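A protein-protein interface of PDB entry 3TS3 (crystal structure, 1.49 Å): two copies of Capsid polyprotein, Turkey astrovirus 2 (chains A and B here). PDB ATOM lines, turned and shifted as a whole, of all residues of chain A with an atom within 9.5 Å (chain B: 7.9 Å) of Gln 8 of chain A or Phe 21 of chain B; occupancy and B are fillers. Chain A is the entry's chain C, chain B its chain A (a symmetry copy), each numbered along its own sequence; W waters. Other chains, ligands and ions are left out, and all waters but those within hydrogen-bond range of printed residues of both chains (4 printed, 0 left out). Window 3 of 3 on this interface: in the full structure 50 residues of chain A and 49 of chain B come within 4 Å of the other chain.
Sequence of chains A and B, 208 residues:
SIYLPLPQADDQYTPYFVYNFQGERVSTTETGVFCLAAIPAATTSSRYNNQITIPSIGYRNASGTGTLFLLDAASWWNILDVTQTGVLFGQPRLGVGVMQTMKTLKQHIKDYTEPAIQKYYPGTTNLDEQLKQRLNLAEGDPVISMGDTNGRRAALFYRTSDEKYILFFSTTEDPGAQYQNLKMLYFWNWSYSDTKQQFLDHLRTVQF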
ATOM      1  N   SER A   1      -6.554  26.408 -24.479  1.00  0.00           N
ATOM      2  CA  SER A   1      -7.875  25.893 -24.142  1.00  0.00           C
ATOM      3  C   SER A   1      -7.759  24.764 -23.122  1.00  0.00           C
ATOM      4  O   SER A   1      -7.762  25.008 -21.922  1.00  0.00           O
ATOM      5  CB  SER A   1      -8.576  25.395 -25.399  1.00  0.00           C
ATOM      6  OG  SER A   1      -7.850  24.333 -25.981  1.00  0.00           O
ATOM      7  N   ILE A   2      -7.641  23.530 -23.596  1.00  0.00           N
ATOM      8  CA  ILE A   2      -7.453  22.409 -22.685  1.00  0.00           C
ATOM      9  C   ILE A   2      -6.037  22.447 -22.132  1.00  0.00           C
ATOM     10  O   ILE A   2      -5.141  22.977 -22.774  1.00  0.00           O
ATOM     11  CB  ILE A   2      -7.680  21.039 -23.357  1.00  0.00           C
ATOM     12  CG1 ILE A   2      -6.610  20.767 -24.413  1.00  0.00           C
ATOM     13  CG2 ILE A   2      -9.061  20.960 -23.940  1.00  0.00           C
ATOM     14  CD1 ILE A   2      -6.746  19.413 -25.099  1.00  0.00           C
ATOM     15  N   TYR A   3      -5.847  21.913 -20.931  1.00  0.00           N
ATOM     16  CA  TYR A   3      -4.501  21.749 -20.386  1.00  0.00           C
ATOM     17  C   TYR A   3      -4.161  20.269 -20.189  1.00  0.00           C
ATOM     18  O   TYR A   3      -3.027  19.924 -19.924  1.00  0.00           O
ATOM     19  CB  TYR A   3      -4.280  22.559 -19.106  1.00  0.00           C
ATOM     20  CG  TYR A   3      -5.158  22.155 -17.956  1.00  0.00           C
ATOM     21  CD1 TYR A   3      -4.748  21.195 -17.048  1.00  0.00           C
ATOM     22  CD2 TYR A   3      -6.393  22.734 -17.778  1.00  0.00           C
ATOM     23  CE1 TYR A   3      -5.547  20.821 -16.005  1.00  0.00           C
ATOM     24  CE2 TYR A   3      -7.194  22.360 -16.739  1.00  0.00           C
ATOM     25  CZ  TYR A   3      -6.765  21.401 -15.859  1.00  0.00           C
ATOM     26  OH  TYR A   3      -7.566  21.022 -14.824  1.00  0.00           O
ATOM     27  N   LEU A   4      -5.166  19.410 -20.345  1.00  0.00           N
ATOM     28  CA  LEU A   4      -4.981  17.961 -20.291  1.00  0.00           C
ATOM     29  C   LEU A   4      -5.365  17.355 -21.639  1.00  0.00           C
ATOM     30  O   LEU A   4      -6.409  17.676 -22.166  1.00  0.00           O
ATOM     31  CB  LEU A   4      -5.841  17.341 -19.183  1.00  0.00           C
ATOM     32  CG  LEU A   4      -5.510  17.700 -17.736  1.00  0.00           C
ATOM     33  CD1 LEU A   4      -6.463  16.988 -16.814  1.00  0.00           C
ATOM     34  CD2 LEU A   4      -4.071  17.316 -17.400  1.00  0.00           C
ATOM     35  N   PRO A   5      -4.527  16.496 -22.205  1.00  0.00           N
ATOM     36  CA  PRO A   5      -3.259  16.046 -21.615  1.00  0.00           C
ATOM     37  C   PRO A   5      -2.181  17.128 -21.563  1.00  0.00           C
ATOM     38  O   PRO A   5      -2.110  17.973 -22.440  1.00  0.00           O
ATOM     39  CB  PRO A   5      -2.815  14.901 -22.538  1.00  0.00           C
ATOM     40  CG  PRO A   5      -3.873  14.708 -23.541  1.00  0.00           C
ATOM     41  CD  PRO A   5      -4.811  15.860 -23.500  1.00  0.00           C
ATOM     42  N   LEU A   6      -1.315  17.048 -20.560  1.00  0.00           N
ATOM     43  CA  LEU A   6      -0.338  18.092 -20.294  1.00  0.00           C
ATOM     44  C   LEU A   6       0.625  18.383 -21.435  1.00  0.00           C
ATOM     45  O   LEU A   6       0.977  19.520 -21.628  1.00  0.00           O
ATOM     46  CB  LEU A   6       0.438  17.833 -18.997  1.00  0.00           C
ATOM     47  CG  LEU A   6      -0.132  18.348 -17.679  1.00  0.00           C
ATOM     48  CD1 LEU A   6       0.908  18.124 -16.596  1.00  0.00           C
ATOM     49  CD2 LEU A   6      -0.479  19.821 -17.778  1.00  0.00           C
ATOM     50  N   PRO A   7       1.027  17.377 -22.202  1.00  0.00           N
ATOM     51  CA  PRO A   7       1.953  17.635 -23.305  1.00  0.00           C
ATOM     52  C   PRO A   7       1.319  18.598 -24.306  1.00  0.00           C
ATOM     53  O   PRO A   7       2.035  19.288 -25.014  1.00  0.00           O
ATOM     54  CB  PRO A   7       2.160  16.254 -23.918  1.00  0.00           C
ATOM     55  CG  PRO A   7       2.000  15.329 -22.757  1.00  0.00           C
ATOM     56  CD  PRO A   7       0.858  15.932 -21.975  1.00  0.00           C
ATOM     57  N   GLN A   8      -0.009  18.631 -24.359  1.00  0.00           N
ATOM     58  CA  GLN A   8      -0.714  19.491 -25.308  1.00  0.00           C
ATOM     59  C   GLN A   8      -1.064  20.865 -24.751  1.00  0.00           C
ATOM     60  O   GLN A   8      -1.544  21.722 -25.468  1.00  0.00           O
ATOM     61  CB  GLN A   8      -1.972  18.788 -25.830  1.00  0.00           C
ATOM     62  CG  GLN A   8      -1.678  17.389 -26.348  1.00  0.00           C
ATOM     63  CD  GLN A   8      -2.873  16.692 -26.964  1.00  0.00           C
ATOM     64  OE1 GLN A   8      -3.842  17.320 -27.347  1.00  0.00           O
ATOM     65  NE2 GLN A   8      -2.799  15.378 -27.044  1.00  0.00           N
ATOM     66  N   ALA A   9      -0.810  21.073 -23.472  1.00  0.00           N
ATOM     67  CA  ALA A   9      -1.178  22.324 -22.834  1.00  0.00           C
ATOM     68  C   ALA A   9      -0.418  23.508 -23.406  1.00  0.00           C
ATOM     69  O   ALA A   9       0.739  23.391 -23.763  1.00  0.00           O
ATOM     70  CB  ALA A   9      -0.964  22.236 -21.326  1.00  0.00           C
ATOM     71  N   ASP A  10      -1.092  24.649 -23.478  1.00  0.00           N
ATOM     72  CA  ASP A  10      -0.471  25.876 -23.942  1.00  0.00           C
ATOM     73  C   ASP A  10       0.506  26.387 -22.882  1.00  0.00           C
ATOM     74  O   ASP A  10       0.363  26.097 -21.706  1.00  0.00           O
ATOM     75  CB  ASP A  10      -1.521  26.951 -24.219  1.00  0.00           C
ATOM     76  CG  ASP A  10      -2.359  26.666 -25.455  1.00  0.00           C
ATOM     77  OD1 ASP A  10      -2.010  25.787 -26.258  1.00  0.00           O
ATOM     78  OD2 ASP A  10      -3.384  27.333 -25.602  1.00  0.00           O
ATOM     79  N   ASP A  11       1.492  27.157 -23.313  1.00  0.00           N
ATOM     80  CA  ASP A  11       2.507  27.662 -22.410  1.00  0.00           C
ATOM     81  C   ASP A  11       1.877  28.621 -21.409  1.00  0.00           C
ATOM     82  O   ASP A  11       0.899  29.284 -21.707  1.00  0.00           O
ATOM     83  CB  ASP A  11       3.626  28.353 -23.194  1.00  0.00           C
ATOM     84  CG  ASP A  11       4.970  28.303 -22.474  1.00  0.00           C
ATOM     85  OD1 ASP A  11       4.999  27.909 -21.298  1.00  0.00           O
ATOM     86  OD2 ASP A  11       5.989  28.635 -23.103  1.00  0.00           O
ATOM     87  N   THR A  83      11.279  15.111 -22.508  1.00  0.00           N
ATOM     88  CA  THR A  83      10.643  16.334 -22.971  1.00  0.00           C
ATOM     89  C   THR A  83       9.124  16.291 -23.121  1.00  0.00           C
ATOM     90  O   THR A  83       8.439  17.213 -22.717  1.00  0.00           O
ATOM     91  CB  THR A  83      11.219  16.746 -24.342  1.00  0.00           C
ATOM     92  OG1 THR A  83      12.648  16.686 -24.299  1.00  0.00           O
ATOM     93  CG2 THR A  83      10.785  18.149 -24.707  1.00  0.00           C
ATOM     94  N   GLN A  84       8.593  15.248 -23.739  1.00  0.00           N
ATOM     95  CA  GLN A  84       7.157  15.214 -23.966  1.00  0.00           C
ATOM     96  C   GLN A  84       6.275  15.122 -22.716  1.00  0.00           C
ATOM     97  O   GLN A  84       5.310  15.856 -22.589  1.00  0.00           O
ATOM     98  CB  GLN A  84       6.789  14.089 -24.944  1.00  0.00           C
ATOM     99  CG  GLN A  84       5.307  14.087 -25.322  1.00  0.00           C
ATOM    100  CD  GLN A  84       4.998  13.202 -26.501  1.00  0.00           C
ATOM    101  OE1 GLN A  84       5.519  12.111 -26.621  1.00  0.00           O
ATOM    102  NE2 GLN A  84       4.131  13.673 -27.371  1.00  0.00           N
ATOM    103  N   THR A  85       6.592  14.189 -21.824  1.00  0.00           N
ATOM    104  CA  THR A  85       5.740  13.950 -20.661  1.00  0.00           C
ATOM    105  C   THR A  85       6.248  14.480 -19.318  1.00  0.00           C
ATOM    106  O   THR A  85       5.531  14.458 -18.336  1.00  0.00           O
ATOM    107  CB  THR A  85       5.432  12.454 -20.515  1.00  0.00           C
ATOM    108  OG1 THR A  85       6.590  11.761 -20.039  1.00  0.00           O
ATOM    109  CG2 THR A  85       5.024  11.879 -21.856  1.00  0.00           C
ATOM    110  N   THR A 101       5.888  22.167 -16.346  1.00  0.00           N
ATOM    111  CA  THR A 101       5.966  21.160 -17.376  1.00  0.00           C
ATOM    112  C   THR A 101       7.330  21.404 -17.999  1.00  0.00           C
ATOM    113  O   THR A 101       7.980  22.383 -17.695  1.00  0.00           O
ATOM    114  CB  THR A 101       4.905  21.301 -18.451  1.00  0.00           C
ATOM    115  OG1 THR A 101       5.017  22.583 -19.061  1.00  0.00           O
ATOM    116  CG2 THR A 101       3.520  21.147 -17.861  1.00  0.00           C
ATOM    117  N   LYS A 103       7.759  22.246 -20.961  1.00  0.00           N
ATOM    118  CA  LYS A 103       7.584  23.456 -21.752  1.00  0.00           C
ATOM    119  C   LYS A 103       7.725  24.742 -20.939  1.00  0.00           C
ATOM    120  O   LYS A 103       8.455  25.637 -21.318  1.00  0.00           O
ATOM    121  CB  LYS A 103       6.209  23.439 -22.423  1.00  0.00           C
ATOM    122  CG  LYS A 103       5.896  24.695 -23.208  1.00  0.00           C
ATOM    123  CD  LYS A 103       4.455  24.739 -23.661  1.00  0.00           C
ATOM    124  CE  LYS A 103       4.173  23.702 -24.713  1.00  0.00           C
ATOM    125  NZ  LYS A 103       2.826  23.963 -25.290  1.00  0.00           N
ATOM    126  N   TYR B   3      -3.203  26.945 -15.423  1.00  0.00           N
ATOM    127  CA  TYR B   3      -3.342  25.607 -14.872  1.00  0.00           C
ATOM    128  C   TYR B   3      -2.215  25.171 -13.921  1.00  0.00           C
ATOM    129  O   TYR B   3      -2.282  24.100 -13.371  1.00  0.00           O
ATOM    130  CB  TYR B   3      -3.502  24.592 -16.009  1.00  0.00           C
ATOM    131  CG  TYR B   3      -2.344  24.613 -16.969  1.00  0.00           C
ATOM    132  CD1 TYR B   3      -1.301  23.714 -16.844  1.00  0.00           C
ATOM    133  CD2 TYR B   3      -2.283  25.542 -17.987  1.00  0.00           C
ATOM    134  CE1 TYR B   3      -0.238  23.735 -17.707  1.00  0.00           C
ATOM    135  CE2 TYR B   3      -1.222  25.569 -18.850  1.00  0.00           C
ATOM    136  CZ  TYR B   3      -0.199  24.668 -18.702  1.00  0.00           C
ATOM    137  OH  TYR B   3       0.861  24.700 -19.570  1.00  0.00           O
ATOM    138  N   TYR B  19      -7.156   7.843 -22.000  1.00  0.00           N
ATOM    139  CA  TYR B  19      -7.436   8.190 -23.394  1.00  0.00           C
ATOM    140  C   TYR B  19      -6.154   8.508 -24.162  1.00  0.00           C
ATOM    141  O   TYR B  19      -5.110   8.746 -23.577  1.00  0.00           O
ATOM    142  CB  TYR B  19      -8.435   9.352 -23.462  1.00  0.00           C
ATOM    143  CG  TYR B  19      -7.951  10.564 -22.726  1.00  0.00           C
ATOM    144  CD1 TYR B  19      -8.225  10.744 -21.383  1.00  0.00           C
ATOM    145  CD2 TYR B  19      -7.191  11.514 -23.365  1.00  0.00           C
ATOM    146  CE1 TYR B  19      -7.766  11.845 -20.719  1.00  0.00           C
ATOM    147  CE2 TYR B  19      -6.731  12.613 -22.702  1.00  0.00           C
ATOM    148  CZ  TYR B  19      -7.019  12.775 -21.379  1.00  0.00           C
ATOM    149  OH  TYR B  19      -6.548  13.879 -20.711  1.00  0.00           O
ATOM    150  N   ASN B  20      -6.242   8.480 -25.485  1.00  0.00           N
ATOM    151  CA  ASN B  20      -5.088   8.746 -26.339  1.00  0.00           C
ATOM    152  C   ASN B  20      -4.923  10.205 -26.756  1.00  0.00           C
ATOM    153  O   ASN B  20      -5.624  11.079 -26.277  1.00  0.00           O
ATOM    154  CB  ASN B  20      -5.034   7.788 -27.538  1.00  0.00           C
ATOM    155  CG  ASN B  20      -6.033   8.124 -28.612  1.00  0.00           C
ATOM    156  OD1 ASN B  20      -6.788   9.078 -28.506  1.00  0.00           O
ATOM    157  ND2 ASN B  20      -6.032   7.326 -29.660  1.00  0.00           N
ATOM    158  N   PHE B  21      -4.014  10.436 -27.690  1.00  0.00           N
ATOM    159  CA  PHE B  21      -3.653  11.783 -28.103  1.00  0.00           C
ATOM    160  C   PHE B  21      -4.836  12.570 -28.650  1.00  0.00           C
ATOM    161  O   PHE B  21      -4.831  13.795 -28.613  1.00  0.00           O
ATOM    162  CB  PHE B  21      -2.498  11.761 -29.121  1.00  0.00           C
ATOM    163  CG  PHE B  21      -2.901  11.304 -30.496  1.00  0.00           C
ATOM    164  CD1 PHE B  21      -2.958  12.199 -31.554  1.00  0.00           C
ATOM    165  CD2 PHE B  21      -3.216   9.983 -30.732  1.00  0.00           C
ATOM    166  CE1 PHE B  21      -3.334  11.775 -32.811  1.00  0.00           C
ATOM    167  CE2 PHE B  21      -3.593   9.565 -31.985  1.00  0.00           C
ATOM    168  CZ  PHE B  21      -3.646  10.464 -33.023  1.00  0.00           C
ATOM    169  N   GLN B  22      -5.837  11.873 -29.170  1.00  0.00           N
ATOM    170  CA  GLN B  22      -7.029  12.553 -29.684  1.00  0.00           C
ATOM    171  C   GLN B  22      -8.321  12.317 -28.906  1.00  0.00           C
ATOM    172  O   GLN B  22      -9.405  12.525 -29.422  1.00  0.00           O
ATOM    173  CB  GLN B  22      -7.215  12.381 -31.195  1.00  0.00           C
ATOM    174  CG  GLN B  22      -7.358  10.981 -31.695  1.00  0.00           C
ATOM    175  CD  GLN B  22      -7.263  10.906 -33.222  1.00  0.00           C
ATOM    176  OE1 GLN B  22      -7.382  11.916 -33.906  1.00  0.00           O
ATOM    177  NE2 GLN B  22      -7.041   9.711 -33.744  1.00  0.00           N
ATOM    178  N   GLY B  23      -8.190  11.908 -27.648  1.00  0.00           N
ATOM    179  CA  GLY B  23      -9.344  11.725 -26.795  1.00  0.00           C
ATOM    180  C   GLY B  23     -10.108  10.422 -26.932  1.00  0.00           C
ATOM    181  O   GLY B  23     -11.193  10.307 -26.394  1.00  0.00           O
ATOM    182  N   GLU B  24      -9.551   9.454 -27.649  1.00  0.00           N
ATOM    183  CA  GLU B  24     -10.193   8.152 -27.809  1.00  0.00           C
ATOM    184  C   GLU B  24      -9.933   7.238 -26.624  1.00  0.00           C
ATOM    185  O   GLU B  24      -8.872   7.283 -26.035  1.00  0.00           O
ATOM    186  CB  GLU B  24      -9.753   7.485 -29.104  1.00  0.00           C
ATOM    187  CG  GLU B  24     -10.121   8.286 -30.316  1.00  0.00           C
ATOM    188  CD  GLU B  24      -9.468   7.769 -31.569  1.00  0.00           C
ATOM    189  OE1 GLU B  24      -8.263   7.489 -31.548  1.00  0.00           O
ATOM    190  OE2 GLU B  24     -10.170   7.666 -32.584  1.00  0.00           O
ATOM    191  N   VAL B  26      -9.085   4.293 -24.065  1.00  0.00           N
ATOM    192  CA  VAL B  26      -8.094   3.238 -23.936  1.00  0.00           C
ATOM    193  C   VAL B  26      -8.544   2.306 -22.812  1.00  0.00           C
ATOM    194  O   VAL B  26      -8.858   2.759 -21.734  1.00  0.00           O
ATOM    195  CB  VAL B  26      -6.708   3.808 -23.611  1.00  0.00           C
ATOM    196  CG1 VAL B  26      -5.748   2.704 -23.252  1.00  0.00           C
ATOM    197  CG2 VAL B  26      -6.178   4.641 -24.768  1.00  0.00           C
ATOM    198  N   LEU B  94       1.298   5.327 -25.541  1.00  0.00           N
ATOM    199  CA  LEU B  94       0.406   6.430 -25.879  1.00  0.00           C
ATOM    200  C   LEU B  94       1.097   7.765 -26.141  1.00  0.00           C
ATOM    201  O   LEU B  94       0.628   8.557 -26.938  1.00  0.00           O
ATOM    202  CB  LEU B  94      -0.693   6.599 -24.830  1.00  0.00           C
ATOM    203  CG  LEU B  94      -1.587   5.385 -24.592  1.00  0.00           C
ATOM    204  CD1 LEU B  94      -2.548   5.707 -23.459  1.00  0.00           C
ATOM    205  CD2 LEU B  94      -2.366   5.008 -25.846  1.00  0.00           C
ATOM    206  N   GLY B  95       2.181   8.026 -25.424  1.00  0.00           N
ATOM    207  CA  GLY B  95       2.864   9.304 -25.525  1.00  0.00           C
ATOM    208  C   GLY B  95       1.940  10.439 -25.120  1.00  0.00           C
ATOM    209  O   GLY B  95       2.036  11.550 -25.621  1.00  0.00           O
ATOM    210  N   VAL B  96       0.999  10.126 -24.239  1.00  0.00           N
ATOM    211  CA  VAL B  96      -0.016  11.080 -23.808  1.00  0.00           C
ATOM    212  C   VAL B  96       0.346  11.886 -22.545  1.00  0.00           C
ATOM    213  O   VAL B  96      -0.194  12.951 -22.301  1.00  0.00           O
ATOM    214  CB  VAL B  96      -1.397  10.370 -23.666  1.00  0.00           C
ATOM    215  CG1 VAL B  96      -1.454   9.505 -22.428  1.00  0.00           C
ATOM    216  CG2 VAL B  96      -2.509  11.368 -23.667  1.00  0.00           C
ATOM    217  N   GLY B  97       1.288  11.375 -21.766  1.00  0.00           N
ATOM    218  CA  GLY B  97       1.708  12.024 -20.532  1.00  0.00           C
ATOM    219  C   GLY B  97       0.634  12.122 -19.454  1.00  0.00           C
ATOM    220  O   GLY B  97      -0.157  11.208 -19.290  1.00  0.00           O
ATOM    221  N   VAL B  98       0.609  13.227 -18.721  1.00  0.00           N
ATOM    222  CA  VAL B  98      -0.376  13.385 -17.659  1.00  0.00           C
ATOM    223  C   VAL B  98      -1.742  13.664 -18.276  1.00  0.00           C
ATOM    224  O   VAL B  98      -1.908  14.620 -19.005  1.00  0.00           O
ATOM    225  CB  VAL B  98       0.010  14.545 -16.716  1.00  0.00           C
ATOM    226  CG1 VAL B  98      -1.157  14.921 -15.791  1.00  0.00           C
ATOM    227  CG2 VAL B  98       1.222  14.162 -15.893  1.00  0.00           C
HETATM  228  O   HOH W   1       3.115  23.379 -20.637  1.00  0.00           O
HETATM  229  O   HOH W   2      -0.937  14.325 -25.210  1.00  0.00           O
HETATM  230  O   HOH W   3       2.884  15.090 -19.071  1.00  0.00           O
HETATM  231  O   HOH W   4       0.678  13.419 -27.023  1.00  0.00           O
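The backbone NH (N) of Leu 6 of chain A is in hydrogen-bond range of the backbone carbonyl oxygen (O) of Val 98 of chain B, 2.9 Å away.
The side-chain amide nitrogen (NE2) of Gln 8 of chain A sits at hydrogen-bond distance from the backbone carbonyl oxygen (O) of Phe 21 of chain B (3.0 Å).
OH of Tyr 3 of chain B is in hydrogen-bond range of O of Asp 10 of chain A, at 2.6 Å.
The side-chain amide nitrogen (NE2) of Gln 84 of chain A sits at hydrogen-bond distance from the backbone carbonyl oxygen (O) of Gly 95 of chain B (3.5 Å).
N of Ser 1 of chain A lies within hydrogen-bond range of OD2 of Asp 10 of chain A, at 3.5 Å.
The backbone carbonyl oxygen (O) of Ala 9 of chain A sits at hydrogen-bond distance from the side-chain amino group (NZ) of Lys 103 of chain A (2.6 Å).
Tyr 19 of chain B touches Leu 4 of chain A (OH to C, 3.8 Å).
Val 98 of chain B touches Leu 4 of chain A.
OH of Tyr 19 of chain B touches N of Pro 5 of chain A, at 3.6 Å.
Pro 5 of chain A touches Val 96 of chain B.
CA of Pro 5 of chain A touches O of Val 98 of chain B (3.3 Å).
CD2 of Leu 6 of chain A touches CE1 of Tyr 3 of chain B, 3.9 Å away.
Pro 7 of chain A touches Val 96 of chain B (CD to O, 3.2 Å).
Pro 7 of chain A touches Gly 97 of chain B.
Ala 9 of chain A touches Tyr 3 of chain B.
Thr 85 of chain A touches Gly 97 of chain B (CG2 to CA, 3.6 Å).
Printed residues of chain B within 4 Å of Leu 4 of chain A: Tyr 19 and Val 98.
Printed residues of chain B within 4 Å of Pro 5 of chain A: Tyr 19 (3.6 Å), Val 96 (3.3 Å) and Val 98 (3.3 Å).
Printed residues of chain B within 4 Å of Leu 6 of chain A: Tyr 3 (3.9 Å) and Val 98 (2.9 Å).
Of the printed residues of chain B, Gln 8 of chain A touches Phe 21.
Of chain B, only Tyr 3 (3.5 Å) comes within 4 Å of Ala 9 of chain A.
Asp 11 of chain A touches none of the printed residues of chain B.
Lys 103 of chain A touches none of the printed residues of chain B.
Phe 21 of chain B touches just one residue of chain A: Gln 8 (3.0 Å).
No residue of chain A comes within 4 Å of Gln 22 of chain B.
Of the printed residues of chain A, Gly 97 of chain B touches Pro 7 and Thr 85.
Of the printed residues of chain A, Val 98 of chain B touches Leu 4, Pro 5 and Leu 6.
The nearest residue of chain B that does not touch Gln 8 of chain A is Gln 22 of chain B (5.1 Å).
The nearest residue of chain A that does not touch Phe 21 of chain B is Pro 5 of chain A (5.2 Å).
Hydrophobic or aromatic side chains of chain B that line the printed part of chain A: Tyr 3, Tyr 19, Val 96 and Val 98.
Hydrophobic or aromatic side chains of chain A that line the printed part of chain B: Tyr 3, Leu 4, Pro 5, Leu 6, Pro 7 and Ala 9.
Along chain A the printed residues that touch a printed residue of chain B span positions 3 to 85.
Among the printed residues, 15 pairs touch across the chains.
Among the printed residues, no Asp or Glu carboxylate lies within 4 Å of a Lys or Arg side-chain nitrogen of the other chain.
Tyr 3 of chain A touches its own counterpart, Tyr 3 of chain B.
Position printed for both chains: 3.
Of the 15 pairs that touch across the chains among the printed residues, 1 has its exchanged pair printed and touching as well.
Water W1 lies within hydrogen-bond range of the side-chain hydroxyl (OG1) of Thr 101 of chain A (2.6 Å) and the side-chain hydroxyl (OH) of Tyr 3 of chain B (2.8 Å).
Water W4 bridges the backbone carbonyl oxygen (O) of Gly 95 of chain B and the side-chain amide nitrogen (NE2) of Gln 84 of chain A.
Water W2 bridges NE2 of Gln 8 of chain A and O of Val 96 of chain B.
Water W3 bridges the backbone carbonyl oxygen (O) of Thr 85 of chain A (2.8 Å) and the backbone NH (N) of Val 98 of chain B (3.0 Å).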
